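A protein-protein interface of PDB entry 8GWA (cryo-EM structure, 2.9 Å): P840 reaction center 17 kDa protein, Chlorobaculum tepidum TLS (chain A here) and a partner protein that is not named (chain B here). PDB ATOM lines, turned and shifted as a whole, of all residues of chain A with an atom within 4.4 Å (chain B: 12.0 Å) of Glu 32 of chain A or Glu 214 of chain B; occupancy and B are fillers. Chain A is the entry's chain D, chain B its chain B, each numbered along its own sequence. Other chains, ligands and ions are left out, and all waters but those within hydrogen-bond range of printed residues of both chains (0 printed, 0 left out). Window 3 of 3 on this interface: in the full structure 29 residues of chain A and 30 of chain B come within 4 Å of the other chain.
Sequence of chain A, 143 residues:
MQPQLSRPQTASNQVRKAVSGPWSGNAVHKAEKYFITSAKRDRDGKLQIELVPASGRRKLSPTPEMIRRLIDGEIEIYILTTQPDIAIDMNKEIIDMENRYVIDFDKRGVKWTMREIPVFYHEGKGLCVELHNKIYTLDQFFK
Among the printed residues, merely in contact across the chains: Gly 25 of chain A with Glu 214 of chain B (3.1 Å), Gly 25 of chain A with Pro 212 of chain B (3.2 Å), Asn 26 of chain A with Thr 211 of chain B (3.4 Å), Ser 24 of chain A with Arg 215 of chain B (3.5 Å), Lys 33 of chain A with Leu 139 of chain B (3.6 Å), Gly 25 of chain A with Thr 211 of chain B (3.9 Å) and Asn 26 of chain A with Glu 214 of chain B (3.99 Å).
Ser 24 of chain A touches two residues of chain B. Gly 25 of chain A touches three residues of chain B. Of the printed residues of chain B, Asn 26 of chain A touches Asp 207 (3.4 Å), Thr 211 (3.4 Å) and Glu 214 (3.99 Å). No residue of chain B comes within 4 Å of Ala 31 of chain A. Glu 32 of chain A touches just one residue of chain B: Glu 214. No residue of chain B comes within 4 Å of Ile 75 of chain A. No residue of chain B comes within 4 Å of Glu 76 of chain A. Printed residues of chain A within 4 Å of Leu 139 of chain B: Lys 33. Of the printed residues of chain A, Asp 207 of chain B touches Asn 26 (3.4 Å). Of the printed residues of chain A, Pro 212 of chain B touches Gly 25. Printed residues of chain A within 4 Å of Glu 214 of chain B: Ser 24, Gly 25, Asn 26 and Glu 32. Leu 216 of chain B touches none of the printed residues of chain A.
Along chain A the printed residues that touch a printed residue of chain B span positions 24 to 33. Hydrophobic or aromatic side chains of chain B within 4 Å of the printed part of chain A: Leu 139 and Pro 212. Along chain B the printed residues that touch a printed residue of chain A span positions 139 to 215. Among the printed residues, 10 pairs touch across the chains.
The backbone NH (N) of Glu 32 of chain A is in hydrogen-bond range of the backbone carbonyl oxygen (O) of Glu 74 of chain A, at 3.3 Å. The side-chain hydroxyl of Tyr 34 of chain A is in hydrogen-bond range of the side-chain carboxylate of Glu 32 of chain A (2.7 Å). O of Glu 32 of chain A is in hydrogen-bond range of N of Glu 76 of chain A, at 2.7 Å.
OD2 of Asp 207 of chain B lies within hydrogen-bond range of ND2 of Asn 26 of chain A (3.4 Å). The side-chain carboxylate of Glu 214 of chain B sits close to the side-chain carboxylate of Glu 32 of chain A (3.4 Å). O of Ser 24 of chain A sits close to OE2 of Glu 214 of chain B (3.4 Å).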
ATOM      1  N   SER A  24     -32.181  10.281  19.611  1.00  0.00           N
ATOM      2  CA  SER A  24     -32.499   9.407  18.485  1.00  0.00           C
ATOM      3  C   SER A  24     -31.623   9.865  17.322  1.00  0.00           C
ATOM      4  O   SER A  24     -31.996  10.752  16.554  1.00  0.00           O
ATOM      5  CB  SER A  24     -33.982   9.467  18.136  1.00  0.00           C
ATOM      6  OG  SER A  24     -34.274  10.606  17.346  1.00  0.00           O
ATOM      7  N   GLY A  25     -30.458   9.248  17.198  1.00  0.00           N
ATOM      8  CA  GLY A  25     -29.470   9.694  16.241  1.00  0.00           C
ATOM      9  C   GLY A  25     -28.510  10.697  16.846  1.00  0.00           C
ATOM     10  O   GLY A  25     -28.438  10.894  18.062  1.00  0.00           O
ATOM     11  N   ASN A  26     -27.756  11.344  15.963  1.00  0.00           N
ATOM     12  CA  ASN A  26     -26.791  12.344  16.397  1.00  0.00           C
ATOM     13  C   ASN A  26     -27.505  13.542  17.010  1.00  0.00           C
ATOM     14  O   ASN A  26     -28.498  14.036  16.472  1.00  0.00           O
ATOM     15  CB  ASN A  26     -25.928  12.792  15.219  1.00  0.00           C
ATOM     16  CG  ASN A  26     -24.486  13.034  15.611  1.00  0.00           C
ATOM     17  OD1 ASN A  26     -24.010  12.515  16.620  1.00  0.00           O
ATOM     18  ND2 ASN A  26     -23.780  13.821  14.810  1.00  0.00           N
ATOM     19  N   ALA A  31     -32.402  17.565  12.275  1.00  0.00           N
ATOM     20  CA  ALA A  31     -32.923  16.735  11.203  1.00  0.00           C
ATOM     21  C   ALA A  31     -31.784  15.925  10.600  1.00  0.00           C
ATOM     22  O   ALA A  31     -30.623  16.343  10.639  1.00  0.00           O
ATOM     23  CB  ALA A  31     -33.598  17.582  10.119  1.00  0.00           C
ATOM     24  N   GLU A  32     -32.122  14.757  10.057  1.00  0.00           N
ATOM     25  CA  GLU A  32     -31.107  13.869   9.506  1.00  0.00           C
ATOM     26  C   GLU A  32     -30.296  14.582   8.434  1.00  0.00           C
ATOM     27  O   GLU A  32     -30.853  15.210   7.529  1.00  0.00           O
ATOM     28  CB  GLU A  32     -31.758  12.612   8.932  1.00  0.00           C
ATOM     29  CG  GLU A  32     -31.883  11.473   9.929  1.00  0.00           C
ATOM     30  CD  GLU A  32     -32.475  10.223   9.312  1.00  0.00           C
ATOM     31  OE1 GLU A  32     -32.482   9.173   9.986  1.00  0.00           O
ATOM     32  OE2 GLU A  32     -32.935  10.292   8.152  1.00  0.00           O
ATOM     33  N   LYS A  33     -28.976  14.485   8.541  1.00  0.00           N
ATOM     34  CA  LYS A  33     -28.065  15.230   7.686  1.00  0.00           C
ATOM     35  C   LYS A  33     -27.442  14.295   6.658  1.00  0.00           C
ATOM     36  O   LYS A  33     -26.779  13.317   7.020  1.00  0.00           O
ATOM     37  CB  LYS A  33     -26.987  15.909   8.531  1.00  0.00           C
ATOM     38  CG  LYS A  33     -26.037  16.811   7.771  1.00  0.00           C
ATOM     39  CD  LYS A  33     -25.083  17.481   8.743  1.00  0.00           C
ATOM     40  CE  LYS A  33     -24.099  18.398   8.048  1.00  0.00           C
ATOM     41  NZ  LYS A  33     -23.178  19.038   9.029  1.00  0.00           N
ATOM     42  N   TYR A  34     -27.655  14.602   5.382  1.00  0.00           N
ATOM     43  CA  TYR A  34     -27.114  13.831   4.274  1.00  0.00           C
ATOM     44  C   TYR A  34     -26.096  14.668   3.513  1.00  0.00           C
ATOM     45  O   TYR A  34     -26.177  15.898   3.481  1.00  0.00           O
ATOM     46  CB  TYR A  34     -28.224  13.357   3.325  1.00  0.00           C
ATOM     47  CG  TYR A  34     -29.213  12.402   3.959  1.00  0.00           C
ATOM     48  CD1 TYR A  34     -28.948  11.041   4.017  1.00  0.00           C
ATOM     49  CD2 TYR A  34     -30.403  12.859   4.502  1.00  0.00           C
ATOM     50  CE1 TYR A  34     -29.842  10.161   4.593  1.00  0.00           C
ATOM     51  CE2 TYR A  34     -31.301  11.986   5.084  1.00  0.00           C
ATOM     52  CZ  TYR A  34     -31.018  10.640   5.126  1.00  0.00           C
ATOM     53  OH  TYR A  34     -31.911   9.766   5.704  1.00  0.00           O
ATOM     54  N   ARG A  69     -39.337  14.063   1.820  1.00  0.00           N
ATOM     55  CA  ARG A  69     -38.867  14.145   3.199  1.00  0.00           C
ATOM     56  C   ARG A  69     -38.043  15.407   3.433  1.00  0.00           C
ATOM     57  O   ARG A  69     -38.032  15.943   4.547  1.00  0.00           O
ATOM     58  CB  ARG A  69     -38.069  12.884   3.541  1.00  0.00           C
ATOM     59  CG  ARG A  69     -37.733  12.720   5.011  1.00  0.00           C
ATOM     60  CD  ARG A  69     -37.168  11.335   5.301  1.00  0.00           C
ATOM     61  NE  ARG A  69     -35.932  11.072   4.574  1.00  0.00           N
ATOM     62  CZ  ARG A  69     -35.308   9.901   4.557  1.00  0.00           C
ATOM     63  NH1 ARG A  69     -35.780   8.855   5.215  1.00  0.00           N
ATOM     64  NH2 ARG A  69     -34.180   9.778   3.863  1.00  0.00           N
ATOM     65  N   GLU A  74     -37.668  17.331   7.344  1.00  0.00           N
ATOM     66  CA  GLU A  74     -37.197  16.188   8.114  1.00  0.00           C
ATOM     67  C   GLU A  74     -35.740  15.831   7.868  1.00  0.00           C
ATOM     68  O   GLU A  74     -35.126  15.204   8.733  1.00  0.00           O
ATOM     69  CB  GLU A  74     -38.059  14.949   7.827  1.00  0.00           C
ATOM     70  CG  GLU A  74     -39.461  15.021   8.402  1.00  0.00           C
ATOM     71  CD  GLU A  74     -40.429  14.103   7.687  1.00  0.00           C
ATOM     72  OE1 GLU A  74     -41.604  14.489   7.519  1.00  0.00           O
ATOM     73  OE2 GLU A  74     -40.015  12.990   7.298  1.00  0.00           O
ATOM     74  N   ILE A  75     -35.175  16.186   6.714  1.00  0.00           N
ATOM     75  CA  ILE A  75     -33.784  15.889   6.405  1.00  0.00           C
ATOM     76  C   ILE A  75     -33.128  17.124   5.803  1.00  0.00           C
ATOM     77  O   ILE A  75     -33.795  18.044   5.326  1.00  0.00           O
ATOM     78  CB  ILE A  75     -33.638  14.689   5.446  1.00  0.00           C
ATOM     79  CG1 ILE A  75     -34.305  14.992   4.105  1.00  0.00           C
ATOM     80  CG2 ILE A  75     -34.236  13.436   6.066  1.00  0.00           C
ATOM     81  CD1 ILE A  75     -34.011  13.970   3.036  1.00  0.00           C
ATOM     82  N   GLU A  76     -31.797  17.132   5.836  1.00  0.00           N
ATOM     83  CA  GLU A  76     -30.999  18.215   5.278  1.00  0.00           C
ATOM     84  C   GLU A  76     -29.861  17.634   4.453  1.00  0.00           C
ATOM     85  O   GLU A  76     -29.313  16.581   4.790  1.00  0.00           O
ATOM     86  CB  GLU A  76     -30.445  19.122   6.379  1.00  0.00           C
ATOM     87  CG  GLU A  76     -31.513  19.909   7.118  1.00  0.00           C
ATOM     88  CD  GLU A  76     -30.939  20.783   8.212  1.00  0.00           C
ATOM     89  OE1 GLU A  76     -29.723  20.682   8.477  1.00  0.00           O
ATOM     90  OE2 GLU A  76     -31.704  21.569   8.809  1.00  0.00           O
ATOM     91  N   LEU B 139     -19.515  24.081  11.037  1.00  0.00           N
ATOM     92  CA  LEU B 139     -19.938  23.639  12.354  1.00  0.00           C
ATOM     93  C   LEU B 139     -18.878  23.869  13.416  1.00  0.00           C
ATOM     94  O   LEU B 139     -19.229  24.046  14.586  1.00  0.00           O
ATOM     95  CB  LEU B 139     -20.311  22.149  12.341  1.00  0.00           C
ATOM     96  CG  LEU B 139     -21.721  21.770  11.873  1.00  0.00           C
ATOM     97  CD1 LEU B 139     -22.786  22.340  12.816  1.00  0.00           C
ATOM     98  CD2 LEU B 139     -21.978  22.175  10.438  1.00  0.00           C
ATOM     99  N   GLY B 194     -19.778  18.246  15.320  1.00  0.00           N
ATOM    100  CA  GLY B 194     -19.761  17.414  14.132  1.00  0.00           C
ATOM    101  C   GLY B 194     -19.100  18.063  12.937  1.00  0.00           C
ATOM    102  O   GLY B 194     -19.592  17.930  11.810  1.00  0.00           O
ATOM    103  N   VAL B 205     -19.210   9.933   3.757  1.00  0.00           N
ATOM    104  CA  VAL B 205     -18.865  10.968   4.722  1.00  0.00           C
ATOM    105  C   VAL B 205     -19.476  10.593   6.062  1.00  0.00           C
ATOM    106  O   VAL B 205     -20.704  10.561   6.206  1.00  0.00           O
ATOM    107  CB  VAL B 205     -19.349  12.353   4.274  1.00  0.00           C
ATOM    108  CG1 VAL B 205     -18.885  13.404   5.264  1.00  0.00           C
ATOM    109  CG2 VAL B 205     -18.851  12.662   2.872  1.00  0.00           C
ATOM    110  N   LEU B 206     -18.624  10.322   7.042  1.00  0.00           N
ATOM    111  CA  LEU B 206     -19.081  10.123   8.405  1.00  0.00           C
ATOM    112  C   LEU B 206     -19.252  11.473   9.090  1.00  0.00           C
ATOM    113  O   LEU B 206     -18.931  12.526   8.539  1.00  0.00           O
ATOM    114  CB  LEU B 206     -18.096   9.255   9.186  1.00  0.00           C
ATOM    115  CG  LEU B 206     -18.084   7.750   8.926  1.00  0.00           C
ATOM    116  CD1 LEU B 206     -16.886   7.118   9.610  1.00  0.00           C
ATOM    117  CD2 LEU B 206     -19.371   7.115   9.406  1.00  0.00           C
ATOM    118  N   ASP B 207     -19.792  11.436  10.300  1.00  0.00           N
ATOM    119  CA  ASP B 207     -19.866  12.623  11.135  1.00  0.00           C
ATOM    120  C   ASP B 207     -19.410  12.360  12.561  1.00  0.00           C
ATOM    121  O   ASP B 207     -18.835  13.259  13.185  1.00  0.00           O
ATOM    122  CB  ASP B 207     -21.307  13.160  11.150  1.00  0.00           C
ATOM    123  CG  ASP B 207     -21.434  14.514  11.811  1.00  0.00           C
ATOM    124  OD1 ASP B 207     -20.430  15.062  12.298  1.00  0.00           O
ATOM    125  OD2 ASP B 207     -22.562  15.039  11.837  1.00  0.00           O
ATOM    126  N   PHE B 208     -19.589  11.147  13.069  1.00  0.00           N
ATOM    127  CA  PHE B 208     -19.171  10.772  14.407  1.00  0.00           C
ATOM    128  C   PHE B 208     -18.993   9.262  14.373  1.00  0.00           C
ATOM    129  O   PHE B 208     -19.615   8.575  13.559  1.00  0.00           O
ATOM    130  CB  PHE B 208     -20.203  11.226  15.449  1.00  0.00           C
ATOM    131  CG  PHE B 208     -19.764  11.053  16.874  1.00  0.00           C
ATOM    132  CD1 PHE B 208     -18.865  11.939  17.441  1.00  0.00           C
ATOM    133  CD2 PHE B 208     -20.266  10.029  17.654  1.00  0.00           C
ATOM    134  CE1 PHE B 208     -18.465  11.798  18.753  1.00  0.00           C
ATOM    135  CE2 PHE B 208     -19.869   9.880  18.967  1.00  0.00           C
ATOM    136  CZ  PHE B 208     -18.970  10.767  19.516  1.00  0.00           C
ATOM    137  N   TYR B 210     -19.794   6.600  16.053  1.00  0.00           N
ATOM    138  CA  TYR B 210     -21.037   5.845  16.043  1.00  0.00           C
ATOM    139  C   TYR B 210     -22.200   6.799  16.266  1.00  0.00           C
ATOM    140  O   TYR B 210     -22.102   7.749  17.046  1.00  0.00           O
ATOM    141  CB  TYR B 210     -21.061   4.738  17.106  1.00  0.00           C
ATOM    142  CG  TYR B 210     -22.437   4.142  17.285  1.00  0.00           C
ATOM    143  CD1 TYR B 210     -22.936   3.229  16.366  1.00  0.00           C
ATOM    144  CD2 TYR B 210     -23.248   4.509  18.350  1.00  0.00           C
ATOM    145  CE1 TYR B 210     -24.196   2.689  16.508  1.00  0.00           C
ATOM    146  CE2 TYR B 210     -24.513   3.975  18.499  1.00  0.00           C
ATOM    147  CZ  TYR B 210     -24.980   3.064  17.575  1.00  0.00           C
ATOM    148  OH  TYR B 210     -26.238   2.525  17.715  1.00  0.00           O
ATOM    149  N   THR B 211     -23.311   6.528  15.585  1.00  0.00           N
ATOM    150  CA  THR B 211     -24.501   7.352  15.668  1.00  0.00           C
ATOM    151  C   THR B 211     -25.659   6.542  16.237  1.00  0.00           C
ATOM    152  O   THR B 211     -25.850   5.384  15.840  1.00  0.00           O
ATOM    153  CB  THR B 211     -24.879   7.903  14.284  1.00  0.00           C
ATOM    154  OG1 THR B 211     -23.731   8.515  13.685  1.00  0.00           O
ATOM    155  CG2 THR B 211     -25.992   8.930  14.399  1.00  0.00           C
ATOM    156  N   PRO B 212     -26.429   7.094  17.173  1.00  0.00           N
ATOM    157  CA  PRO B 212     -27.586   6.375  17.723  1.00  0.00           C
ATOM    158  C   PRO B 212     -28.544   5.935  16.630  1.00  0.00           C
ATOM    159  O   PRO B 212     -28.527   6.479  15.515  1.00  0.00           O
ATOM    160  CB  PRO B 212     -28.226   7.418  18.650  1.00  0.00           C
ATOM    161  CG  PRO B 212     -27.073   8.224  19.123  1.00  0.00           C
ATOM    162  CD  PRO B 212     -26.093   8.286  17.972  1.00  0.00           C
ATOM    163  N   PRO B 213     -29.409   4.954  16.912  1.00  0.00           N
ATOM    164  CA  PRO B 213     -30.114   4.251  15.830  1.00  0.00           C
ATOM    165  C   PRO B 213     -31.373   4.920  15.292  1.00  0.00           C
ATOM    166  O   PRO B 213     -32.165   4.244  14.629  1.00  0.00           O
ATOM    167  CB  PRO B 213     -30.455   2.899  16.469  1.00  0.00           C
ATOM    168  CG  PRO B 213     -30.552   3.188  17.919  1.00  0.00           C
ATOM    169  CD  PRO B 213     -29.554   4.264  18.207  1.00  0.00           C
ATOM    170  N   GLU B 214     -31.597   6.209  15.567  1.00  0.00           N
ATOM    171  CA  GLU B 214     -32.710   6.955  14.969  1.00  0.00           C
ATOM    172  C   GLU B 214     -34.058   6.302  15.290  1.00  0.00           C
ATOM    173  O   GLU B 214     -34.781   5.843  14.405  1.00  0.00           O
ATOM    174  CB  GLU B 214     -32.529   7.088  13.451  1.00  0.00           C
ATOM    175  CG  GLU B 214     -31.388   7.975  12.974  1.00  0.00           C
ATOM    176  CD  GLU B 214     -31.615   9.441  13.275  1.00  0.00           C
ATOM    177  OE1 GLU B 214     -32.789   9.869  13.295  1.00  0.00           O
ATOM    178  OE2 GLU B 214     -30.623  10.176  13.452  1.00  0.00           O
ATOM    179  N   ARG B 215     -34.393   6.271  16.575  1.00  0.00           N
ATOM    180  CA  ARG B 215     -35.547   5.516  17.040  1.00  0.00           C
ATOM    181  C   ARG B 215     -36.821   6.353  17.040  1.00  0.00           C
ATOM    182  O   ARG B 215     -36.801   7.555  17.315  1.00  0.00           O
ATOM    183  CB  ARG B 215     -35.304   4.982  18.452  1.00  0.00           C
ATOM    184  CG  ARG B 215     -33.909   4.456  18.712  1.00  0.00           C
ATOM    185  CD  ARG B 215     -33.938   3.485  19.878  1.00  0.00           C
ATOM    186  NE  ARG B 215     -35.145   2.667  19.845  1.00  0.00           N
ATOM    187  CZ  ARG B 215     -35.654   2.032  20.892  1.00  0.00           C
ATOM    188  NH1 ARG B 215     -35.081   2.092  22.082  1.00  0.00           N
ATOM    189  NH2 ARG B 215     -36.766   1.320  20.739  1.00  0.00           N
ATOM    190  N   LEU B 216     -37.937   5.699  16.724  1.00  0.00           N
ATOM    191  CA  LEU B 216     -39.246   6.270  17.008  1.00  0.00           C
ATOM    192  C   LEU B 216     -39.496   6.255  18.509  1.00  0.00           C
ATOM    193  O   LEU B 216     -39.203   5.275  19.200  1.00  0.00           O
ATOM    194  CB  LEU B 216     -40.354   5.485  16.305  1.00  0.00           C
ATOM    195  CG  LEU B 216     -40.522   5.572  14.791  1.00  0.00           C
ATOM    196  CD1 LEU B 216     -41.644   4.653  14.346  1.00  0.00           C
ATOM    197  CD2 LEU B 216     -40.798   7.001  14.362  1.00  0.00           C
ATOM    198  N   ASP B 217     -40.054   7.350  19.017  1.00  0.00           N
ATOM    199  CA  ASP B 217     -40.217   7.517  20.452  1.00  0.00           C
ATOM    200  C   ASP B 217     -41.657   7.875  20.781  1.00  0.00           C
ATOM    201  O   ASP B 217     -42.360   8.496  19.979  1.00  0.00           O
ATOM    202  CB  ASP B 217     -39.282   8.604  21.002  1.00  0.00           C
ATOM    203  CG  ASP B 217     -37.809   8.244  20.868  1.00  0.00           C
ATOM    204  OD1 ASP B 217     -37.489   7.140  20.388  1.00  0.00           O
ATOM    205  OD2 ASP B 217     -36.960   9.078  21.245  1.00  0.00           O
ATOM    206  N   PHE B 218     -42.085   7.471  21.975  1.00  0.00           N
ATOM    207  CA  PHE B 218     -43.353   7.911  22.540  1.00  0.00           C
ATOM    208  C   PHE B 218     -43.278   7.774  24.053  1.00  0.00           C
ATOM    209  O   PHE B 218     -42.388   7.112  24.591  1.00  0.00           O
ATOM    210  CB  PHE B 218     -44.548   7.129  21.976  1.00  0.00           C
ATOM    211  CG  PHE B 218     -44.450   5.632  22.140  1.00  0.00           C
ATOM    212  CD1 PHE B 218     -44.661   5.033  23.372  1.00  0.00           C
ATOM    213  CD2 PHE B 218     -44.196   4.823  21.049  1.00  0.00           C
ATOM    214  CE1 PHE B 218     -44.587   3.663  23.516  1.00  0.00           C
ATOM    215  CE2 PHE B 218     -44.125   3.452  21.188  1.00  0.00           C
ATOM    216  CZ  PHE B 218     -44.322   2.873  22.424  1.00  0.00           C
